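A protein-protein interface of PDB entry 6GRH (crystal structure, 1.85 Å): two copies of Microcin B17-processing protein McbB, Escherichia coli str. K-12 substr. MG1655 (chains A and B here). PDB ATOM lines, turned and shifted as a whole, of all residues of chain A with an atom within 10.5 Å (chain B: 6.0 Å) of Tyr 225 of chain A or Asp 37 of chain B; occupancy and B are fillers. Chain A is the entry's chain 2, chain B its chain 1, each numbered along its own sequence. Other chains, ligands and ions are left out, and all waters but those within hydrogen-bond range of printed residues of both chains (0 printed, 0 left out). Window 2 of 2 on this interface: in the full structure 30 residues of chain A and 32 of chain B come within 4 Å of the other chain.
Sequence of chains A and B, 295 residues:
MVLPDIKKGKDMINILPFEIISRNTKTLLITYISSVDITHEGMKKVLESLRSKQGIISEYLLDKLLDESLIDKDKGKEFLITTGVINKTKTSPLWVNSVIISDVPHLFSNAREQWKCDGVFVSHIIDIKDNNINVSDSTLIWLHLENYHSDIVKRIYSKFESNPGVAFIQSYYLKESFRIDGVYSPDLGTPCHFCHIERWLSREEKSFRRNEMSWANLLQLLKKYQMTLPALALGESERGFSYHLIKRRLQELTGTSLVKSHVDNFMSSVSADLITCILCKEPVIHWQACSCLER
Of the 17 printed residues of chain A, 7 touch a printed residue of chain B.
Printed residues of chain A that touch a printed residue of chain B: Trp 215, Leu 218, Leu 221, Leu 222, Tyr 225, Gln 226 and Met 227.
Hydrophobic or aromatic side chains of chain A that line the printed part of chain B: Trp 215, Leu 218, Leu 221, Leu 222, Tyr 225 and Met 227.
Along chain A the printed residues that touch a printed residue of chain B span positions 215 to 227.
Among the printed residues, 10 pairs touch across the chains.
Among the printed residues, pairs that only touch across the chains: Trp 215 of chain A with Ser 35 of chain B (3.9 Å), Leu 218 of chain A with Leu 28 of chain B (3.8 Å), Leu 218 of chain A with Ser 35 of chain B (3.2 Å), Leu 221 of chain A with Leu 28 of chain B (3.9 Å), Leu 222 of chain A with Leu 28 of chain B (3.4 Å), Tyr 225 of chain A with Arg 23 of chain B (3.2 Å), Tyr 225 of chain A with Lys 26 of chain B (3.2 Å), Gln 226 of chain A with Arg 23 of chain B (3.5 Å) and Met 227 of chain A with Arg 23 of chain B (3.7 Å).
Of chain B, only Arg 23 (3.2 Å), Lys 26 (3.2 Å) and Asp 37 (3.1 Å) come within 4 Å of Tyr 225 of chain A.
Asp 37 of chain B touches one residue of chain A.
Arg 23 of chain B touches just these residues of chain A: Tyr 225, Gln 226 and Met 227.
Of the printed residues of chain A, Lys 26 of chain B touches Tyr 225.
No residue of chain A comes within 4 Å of Val 36 of chain B.
Printed residues of chain B within 4 Å of Leu 221 of chain A: Leu 28 (3.9 Å).
Of the printed residues of chain B, Leu 218 of chain A touches Leu 28 (3.8 Å) and Ser 35 (3.2 Å).
Leu 29 of chain B touches none of the printed residues of chain A.
Asp 151 of chain A touches none of the printed residues of chain B.
The nearest residue of chain A that does not touch Asp 37 of chain B is Leu 221 of chain A (4.2 Å).
No position is printed for both chains.
Of the 10 pairs that touch across the chains among the printed residues, none has its exchanged pair printed and touching as well.
O of Leu 222 of chain A is in hydrogen-bond range of N of Met 227 of chain A (2.9 Å).
The side-chain hydroxyl of Ser 35 of chain B lies within hydrogen-bond range of the backbone carbonyl oxygen of Leu 29 of chain B (3.1 Å).
OD2 of Asp 37 of chain B is in hydrogen-bond range of OH of Tyr 225 of chain A (3.1 Å).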
ATOM      1  N   HIS A 149      -0.124  10.073   1.551  1.00  0.00           N
ATOM      2  CA  HIS A 149       1.324  10.131   1.400  1.00  0.00           C
ATOM      3  C   HIS A 149       1.814  11.362   2.129  1.00  0.00           C
ATOM      4  O   HIS A 149       1.223  12.415   2.011  1.00  0.00           O
ATOM      5  CB  HIS A 149       1.727  10.208  -0.070  1.00  0.00           C
ATOM      6  CG  HIS A 149       3.183   9.927  -0.321  1.00  0.00           C
ATOM      7  ND1 HIS A 149       4.179  10.842  -0.060  1.00  0.00           N
ATOM      8  CD2 HIS A 149       3.804   8.841  -0.844  1.00  0.00           C
ATOM      9  CE1 HIS A 149       5.352  10.329  -0.396  1.00  0.00           C
ATOM     10  NE2 HIS A 149       5.149   9.121  -0.890  1.00  0.00           N
ATOM     11  N   ASP A 151       4.276  13.439   1.617  1.00  0.00           N
ATOM     12  CA  ASP A 151       4.593  14.568   0.729  1.00  0.00           C
ATOM     13  C   ASP A 151       3.388  15.428   0.337  1.00  0.00           C
ATOM     14  O   ASP A 151       3.551  16.592   0.010  1.00  0.00           O
ATOM     15  CB  ASP A 151       5.291  14.083  -0.557  1.00  0.00           C
ATOM     16  CG  ASP A 151       6.721  13.600  -0.324  1.00  0.00           C
ATOM     17  OD1 ASP A 151       7.323  13.873   0.727  1.00  0.00           O
ATOM     18  OD2 ASP A 151       7.248  12.938  -1.230  1.00  0.00           O
ATOM     19  N   MET A 213       8.337  -7.220  11.641  1.00  0.00           N
ATOM     20  CA  MET A 213       7.005  -7.101  11.018  1.00  0.00           C
ATOM     21  C   MET A 213       6.262  -5.811  11.427  1.00  0.00           C
ATOM     22  O   MET A 213       5.028  -5.781  11.473  1.00  0.00           O
ATOM     23  CB  MET A 213       6.168  -8.325  11.379  1.00  0.00           C
ATOM     24  CG  MET A 213       6.789  -9.647  10.952  1.00  0.00           C
ATOM     25  SD  MET A 213       6.820  -9.753   9.141  1.00  0.00           S
ATOM     26  CE  MET A 213       8.542 -10.181   8.865  1.00  0.00           C
ATOM     27  N   TRP A 215       4.596  -2.207  11.037  1.00  0.00           N
ATOM     28  CA  TRP A 215       3.882  -1.469  10.008  1.00  0.00           C
ATOM     29  C   TRP A 215       4.691  -0.301   9.468  1.00  0.00           C
ATOM     30  O   TRP A 215       4.370   0.216   8.393  1.00  0.00           O
ATOM     31  CB  TRP A 215       2.510  -1.008  10.511  1.00  0.00           C
ATOM     32  CG  TRP A 215       1.640  -2.169  10.629  1.00  0.00           C
ATOM     33  CD1 TRP A 215       1.504  -2.969  11.716  1.00  0.00           C
ATOM     34  CD2 TRP A 215       0.845  -2.755   9.596  1.00  0.00           C
ATOM     35  NE1 TRP A 215       0.640  -3.985  11.444  1.00  0.00           N
ATOM     36  CE2 TRP A 215       0.234  -3.892  10.141  1.00  0.00           C
ATOM     37  CE3 TRP A 215       0.578  -2.419   8.264  1.00  0.00           C
ATOM     38  CZ2 TRP A 215      -0.628  -4.715   9.400  1.00  0.00           C
ATOM     39  CZ3 TRP A 215      -0.299  -3.227   7.529  1.00  0.00           C
ATOM     40  CH2 TRP A 215      -0.888  -4.360   8.105  1.00  0.00           C
ATOM     41  N   ASN A 217       7.530  -0.842   8.220  1.00  0.00           N
ATOM     42  CA  ASN A 217       8.085  -1.446   7.002  1.00  0.00           C
ATOM     43  C   ASN A 217       7.210  -1.155   5.791  1.00  0.00           C
ATOM     44  O   ASN A 217       7.736  -0.869   4.709  1.00  0.00           O
ATOM     45  CB  ASN A 217       8.236  -2.964   7.111  1.00  0.00           C
ATOM     46  CG  ASN A 217       9.261  -3.377   8.108  1.00  0.00           C
ATOM     47  OD1 ASN A 217      10.129  -2.590   8.473  1.00  0.00           O
ATOM     48  ND2 ASN A 217       9.184  -4.630   8.558  1.00  0.00           N
ATOM     49  N   LEU A 218       5.885  -1.244   5.964  1.00  0.00           N
ATOM     50  CA  LEU A 218       4.967  -0.948   4.882  1.00  0.00           C
ATOM     51  C   LEU A 218       5.066   0.513   4.515  1.00  0.00           C
ATOM     52  O   LEU A 218       5.218   0.847   3.336  1.00  0.00           O
ATOM     53  CB  LEU A 218       3.518  -1.267   5.263  1.00  0.00           C
ATOM     54  CG  LEU A 218       2.480  -0.802   4.243  1.00  0.00           C
ATOM     55  CD1 LEU A 218       2.707  -1.464   2.874  1.00  0.00           C
ATOM     56  CD2 LEU A 218       1.121  -1.128   4.792  1.00  0.00           C
ATOM     57  N   LEU A 219       4.966   1.385   5.515  1.00  0.00           N
ATOM     58  CA  LEU A 219       4.962   2.829   5.259  1.00  0.00           C
ATOM     59  C   LEU A 219       6.243   3.263   4.553  1.00  0.00           C
ATOM     60  O   LEU A 219       6.173   4.021   3.589  1.00  0.00           O
ATOM     61  CB  LEU A 219       4.765   3.657   6.538  1.00  0.00           C
ATOM     62  CG  LEU A 219       3.451   3.488   7.306  1.00  0.00           C
ATOM     63  CD1 LEU A 219       3.434   4.379   8.543  1.00  0.00           C
ATOM     64  CD2 LEU A 219       2.226   3.763   6.466  1.00  0.00           C
ATOM     65  N   GLN A 220       7.390   2.757   5.004  1.00  0.00           N
ATOM     66  CA  GLN A 220       8.684   3.129   4.407  1.00  0.00           C
ATOM     67  C   GLN A 220       8.838   2.507   3.005  1.00  0.00           C
ATOM     68  O   GLN A 220       9.419   3.136   2.126  1.00  0.00           O
ATOM     69  CB  GLN A 220       9.880   2.791   5.330  1.00  0.00           C
ATOM     70  CG  GLN A 220       9.876   3.409   6.760  1.00  0.00           C
ATOM     71  CD  GLN A 220      10.008   4.947   6.843  1.00  0.00           C
ATOM     72  OE1 GLN A 220       9.797   5.671   5.864  1.00  0.00           O
ATOM     73  NE2 GLN A 220      10.350   5.447   8.039  1.00  0.00           N
ATOM     74  N   LEU A 221       8.310   1.301   2.777  1.00  0.00           N
ATOM     75  CA  LEU A 221       8.344   0.702   1.437  1.00  0.00           C
ATOM     76  C   LEU A 221       7.462   1.450   0.430  1.00  0.00           C
ATOM     77  O   LEU A 221       7.830   1.553  -0.746  1.00  0.00           O
ATOM     78  CB  LEU A 221       7.969  -0.791   1.453  1.00  0.00           C
ATOM     79  CG  LEU A 221       8.196  -1.547   0.136  1.00  0.00           C
ATOM     80  CD1 LEU A 221       9.662  -1.475  -0.322  1.00  0.00           C
ATOM     81  CD2 LEU A 221       7.780  -3.002   0.258  1.00  0.00           C
ATOM     82  N   LEU A 222       6.308   1.948   0.881  1.00  0.00           N
ATOM     83  CA  LEU A 222       5.454   2.793   0.047  1.00  0.00           C
ATOM     84  C   LEU A 222       6.157   4.098  -0.364  1.00  0.00           C
ATOM     85  O   LEU A 222       6.062   4.497  -1.524  1.00  0.00           O
ATOM     86  CB  LEU A 222       4.123   3.108   0.737  1.00  0.00           C
ATOM     87  CG  LEU A 222       3.164   1.943   0.984  1.00  0.00           C
ATOM     88  CD1 LEU A 222       2.084   2.367   1.979  1.00  0.00           C
ATOM     89  CD2 LEU A 222       2.547   1.448  -0.302  1.00  0.00           C
ATOM     90  N   LYS A 223       6.875   4.745   0.559  1.00  0.00           N
ATOM     91  CA  LYS A 223       7.784   5.855   0.168  1.00  0.00           C
ATOM     92  C   LYS A 223       8.759   5.417  -0.964  1.00  0.00           C
ATOM     93  O   LYS A 223       8.746   5.982  -2.059  1.00  0.00           O
ATOM     94  CB  LYS A 223       8.567   6.398   1.369  1.00  0.00           C
ATOM     95  N   LYS A 224       9.527   4.351  -0.731  1.00  0.00           N
ATOM     96  CA  LYS A 224      10.522   3.868  -1.695  1.00  0.00           C
ATOM     97  C   LYS A 224       9.903   3.584  -3.071  1.00  0.00           C
ATOM     98  O   LYS A 224      10.483   3.899  -4.100  1.00  0.00           O
ATOM     99  CB  LYS A 224      11.200   2.601  -1.155  1.00  0.00           C
ATOM    100  CG  LYS A 224      12.375   2.092  -1.976  1.00  0.00           C
ATOM    101  CD  LYS A 224      12.809   0.714  -1.507  1.00  0.00           C
ATOM    102  N   TYR A 225       8.711   3.005  -3.074  1.00  0.00           N
ATOM    103  CA  TYR A 225       8.031   2.617  -4.300  1.00  0.00           C
ATOM    104  C   TYR A 225       7.177   3.747  -4.892  1.00  0.00           C
ATOM    105  O   TYR A 225       6.545   3.538  -5.916  1.00  0.00           O
ATOM    106  CB  TYR A 225       7.164   1.386  -4.027  1.00  0.00           C
ATOM    107  CG  TYR A 225       7.882   0.052  -3.870  1.00  0.00           C
ATOM    108  CD1 TYR A 225       9.295  -0.066  -3.850  1.00  0.00           C
ATOM    109  CD2 TYR A 225       7.124  -1.113  -3.710  1.00  0.00           C
ATOM    110  CE1 TYR A 225       9.903  -1.318  -3.711  1.00  0.00           C
ATOM    111  CE2 TYR A 225       7.720  -2.359  -3.574  1.00  0.00           C
ATOM    112  CZ  TYR A 225       9.101  -2.464  -3.569  1.00  0.00           C
ATOM    113  OH  TYR A 225       9.624  -3.730  -3.427  1.00  0.00           O
ATOM    114  N   GLN A 226       7.176   4.925  -4.263  1.00  0.00           N
ATOM    115  CA  GLN A 226       6.430   6.107  -4.713  1.00  0.00           C
ATOM    116  C   GLN A 226       4.900   5.865  -4.757  1.00  0.00           C
ATOM    117  O   GLN A 226       4.208   6.302  -5.679  1.00  0.00           O
ATOM    118  CB  GLN A 226       6.988   6.622  -6.056  1.00  0.00           C
ATOM    119  CG  GLN A 226       8.458   7.040  -5.966  1.00  0.00           C
ATOM    120  CD  GLN A 226       9.112   7.244  -7.325  1.00  0.00           C
ATOM    121  OE1 GLN A 226       9.069   6.370  -8.192  1.00  0.00           O
ATOM    122  NE2 GLN A 226       9.730   8.395  -7.512  1.00  0.00           N
ATOM    123  N   MET A 227       4.396   5.138  -3.767  1.00  0.00           N
ATOM    124  CA  MET A 227       2.977   4.754  -3.719  1.00  0.00           C
ATOM    125  C   MET A 227       2.295   5.416  -2.512  1.00  0.00           C
ATOM    126  O   MET A 227       2.941   5.703  -1.497  1.00  0.00           O
ATOM    127  CB  MET A 227       2.845   3.240  -3.608  1.00  0.00           C
ATOM    128  CG  MET A 227       3.678   2.451  -4.617  1.00  0.00           C
ATOM    129  SD  MET A 227       3.512   0.671  -4.369  1.00  0.00           S
ATOM    130  CE  MET A 227       1.946   0.369  -5.164  1.00  0.00           C
ATOM    131  N   THR A 228       0.998   5.664  -2.646  1.00  0.00           N
ATOM    132  CA  THR A 228       0.168   6.100  -1.537  1.00  0.00           C
ATOM    133  C   THR A 228      -0.350   4.910  -0.704  1.00  0.00           C
ATOM    134  O   THR A 228      -0.423   3.780  -1.180  1.00  0.00           O
ATOM    135  CB  THR A 228      -1.037   6.940  -2.015  1.00  0.00           C
ATOM    136  OG1 THR A 228      -1.780   6.198  -2.978  1.00  0.00           O
ATOM    137  CG2 THR A 228      -0.572   8.234  -2.653  1.00  0.00           C
ATOM    138  N   LEU A 229      -0.660   5.189   0.554  1.00  0.00           N
ATOM    139  CA  LEU A 229      -1.330   4.237   1.438  1.00  0.00           C
ATOM    140  C   LEU A 229      -2.830   4.407   1.218  1.00  0.00           C
ATOM    141  O   LEU A 229      -3.376   5.426   1.597  1.00  0.00           O
ATOM    142  CB  LEU A 229      -1.008   4.525   2.904  1.00  0.00           C
ATOM    143  CG  LEU A 229      -1.716   3.664   3.960  1.00  0.00           C
ATOM    144  CD1 LEU A 229      -1.140   2.268   3.946  1.00  0.00           C
ATOM    145  CD2 LEU A 229      -1.541   4.261   5.343  1.00  0.00           C
ATOM    146  N   ARG B  23       2.447  -0.463  -8.781  1.00  0.00           N
ATOM    147  CA  ARG B  23       3.115   0.615  -9.483  1.00  0.00           C
ATOM    148  C   ARG B  23       4.482   0.110  -9.940  1.00  0.00           C
ATOM    149  O   ARG B  23       5.221  -0.495  -9.143  1.00  0.00           O
ATOM    150  CB  ARG B  23       3.271   1.821  -8.574  1.00  0.00           C
ATOM    151  CG  ARG B  23       3.730   3.077  -9.292  1.00  0.00           C
ATOM    152  CD  ARG B  23       4.453   4.008  -8.336  1.00  0.00           C
ATOM    153  NE  ARG B  23       5.088   5.139  -9.014  1.00  0.00           N
ATOM    154  CZ  ARG B  23       4.489   6.287  -9.345  1.00  0.00           C
ATOM    155  NH1 ARG B  23       3.198   6.507  -9.079  1.00  0.00           N
ATOM    156  NH2 ARG B  23       5.204   7.237  -9.954  1.00  0.00           N
ATOM    157  N   LYS B  26       6.124  -3.259  -8.811  1.00  0.00           N
ATOM    158  CA  LYS B  26       5.861  -3.478  -7.392  1.00  0.00           C
ATOM    159  C   LYS B  26       4.369  -3.679  -7.135  1.00  0.00           C
ATOM    160  O   LYS B  26       3.541  -2.921  -7.634  1.00  0.00           O
ATOM    161  CB  LYS B  26       6.357  -2.274  -6.612  1.00  0.00           C
ATOM    162  N   THR B  27       4.040  -4.701  -6.345  1.00  0.00           N
ATOM    163  CA  THR B  27       2.663  -5.021  -5.982  1.00  0.00           C
ATOM    164  C   THR B  27       2.582  -5.328  -4.501  1.00  0.00           C
ATOM    165  O   THR B  27       3.326  -6.163  -4.009  1.00  0.00           O
ATOM    166  CB  THR B  27       2.154  -6.218  -6.805  1.00  0.00           C
ATOM    167  OG1 THR B  27       2.164  -5.825  -8.168  1.00  0.00           O
ATOM    168  CG2 THR B  27       0.731  -6.596  -6.441  1.00  0.00           C
ATOM    169  N   LEU B  28       1.683  -4.641  -3.806  1.00  0.00           N
ATOM    170  CA  LEU B  28       1.524  -4.818  -2.358  1.00  0.00           C
ATOM    171  C   LEU B  28       0.070  -5.167  -2.016  1.00  0.00           C
ATOM    172  O   LEU B  28      -0.858  -4.536  -2.524  1.00  0.00           O
ATOM    173  CB  LEU B  28       1.935  -3.567  -1.583  1.00  0.00           C
ATOM    174  CG  LEU B  28       3.330  -2.974  -1.774  1.00  0.00           C
ATOM    175  CD1 LEU B  28       3.527  -1.817  -0.808  1.00  0.00           C
ATOM    176  CD2 LEU B  28       4.445  -3.983  -1.569  1.00  0.00           C
ATOM    177  N   LEU B  29      -0.065  -6.177  -1.158  1.00  0.00           N
ATOM    178  CA  LEU B  29      -1.301  -6.594  -0.538  1.00  0.00           C
ATOM    179  C   LEU B  29      -1.308  -5.959   0.845  1.00  0.00           C
ATOM    180  O   LEU B  29      -0.323  -6.081   1.563  1.00  0.00           O
ATOM    181  CB  LEU B  29      -1.317  -8.120  -0.384  1.00  0.00           C
ATOM    182  CG  LEU B  29      -2.454  -8.713   0.450  1.00  0.00           C
ATOM    183  CD1 LEU B  29      -3.779  -8.438  -0.207  1.00  0.00           C
ATOM    184  CD2 LEU B  29      -2.295 -10.185   0.744  1.00  0.00           C
ATOM    185  N   SER B  35       0.673  -7.088   5.715  1.00  0.00           N
ATOM    186  CA  SER B  35       1.022  -6.528   4.435  1.00  0.00           C
ATOM    187  C   SER B  35       2.072  -7.428   3.778  1.00  0.00           C
ATOM    188  O   SER B  35       2.952  -7.944   4.457  1.00  0.00           O
ATOM    189  CB  SER B  35       1.530  -5.104   4.593  1.00  0.00           C
ATOM    190  OG  SER B  35       1.622  -4.487   3.328  1.00  0.00           O
ATOM    191  N   VAL B  36       1.951  -7.618   2.460  1.00  0.00           N
ATOM    192  CA  VAL B  36       2.821  -8.546   1.714  1.00  0.00           C
ATOM    193  C   VAL B  36       3.281  -7.888   0.421  1.00  0.00           C
ATOM    194  O   VAL B  36       2.479  -7.330  -0.314  1.00  0.00           O
ATOM    195  CB  VAL B  36       2.112  -9.891   1.423  1.00  0.00           C
ATOM    196  CG1 VAL B  36       3.063 -10.883   0.747  1.00  0.00           C
ATOM    197  CG2 VAL B  36       1.566 -10.511   2.704  1.00  0.00           C
ATOM    198  N   ASP B  37       4.594  -7.931   0.181  1.00  0.00           N
ATOM    199  CA  ASP B  37       5.155  -7.561  -1.113  1.00  0.00           C
ATOM    200  C   ASP B  37       4.960  -8.787  -2.030  1.00  0.00           C
ATOM    201  O   ASP B  37       5.624  -9.792  -1.853  1.00  0.00           O
ATOM    202  CB  ASP B  37       6.635  -7.179  -0.945  1.00  0.00           C
ATOM    203  CG  ASP B  37       7.258  -6.567  -2.205  1.00  0.00           C
ATOM    204  OD1 ASP B  37       6.551  -6.311  -3.209  1.00  0.00           O
ATOM    205  OD2 ASP B  37       8.493  -6.332  -2.199  1.00  0.00           O
ATOM    206  N   ILE B  38       4.042  -8.696  -2.978  1.00  0.00           N
ATOM    207  CA  ILE B  38       3.630  -9.859  -3.783  1.00  0.00           C
ATOM    208  C   ILE B  38       4.597 -10.029  -4.951  1.00  0.00           C
ATOM    209  O   ILE B  38       4.758  -9.112  -5.751  1.00  0.00           O
ATOM    210  CB  ILE B  38       2.216  -9.679  -4.356  1.00  0.00           C
ATOM    211  CG1 ILE B  38       1.186  -9.535  -3.241  1.00  0.00           C
ATOM    212  CG2 ILE B  38       1.819 -10.847  -5.285  1.00  0.00           C
ATOM    213  CD1 ILE B  38       0.979 -10.771  -2.386  1.00  0.00           C
ATOM    214  N   THR B  39       5.232 -11.185  -5.053  1.00  0.00           N
ATOM    215  CA  THR B  39       6.195 -11.415  -6.146  1.00  0.00           C
ATOM    216  C   THR B  39       5.756 -12.490  -7.143  1.00  0.00           C
ATOM    217  O   THR B  39       6.505 -12.811  -8.022  1.00  0.00           O
ATOM    218  CB  THR B  39       7.585 -11.788  -5.600  1.00  0.00           C
ATOM    219  OG1 THR B  39       7.451 -12.917  -4.717  1.00  0.00           O
ATOM    220  CG2 THR B  39       8.218 -10.570  -4.850  1.00  0.00           C
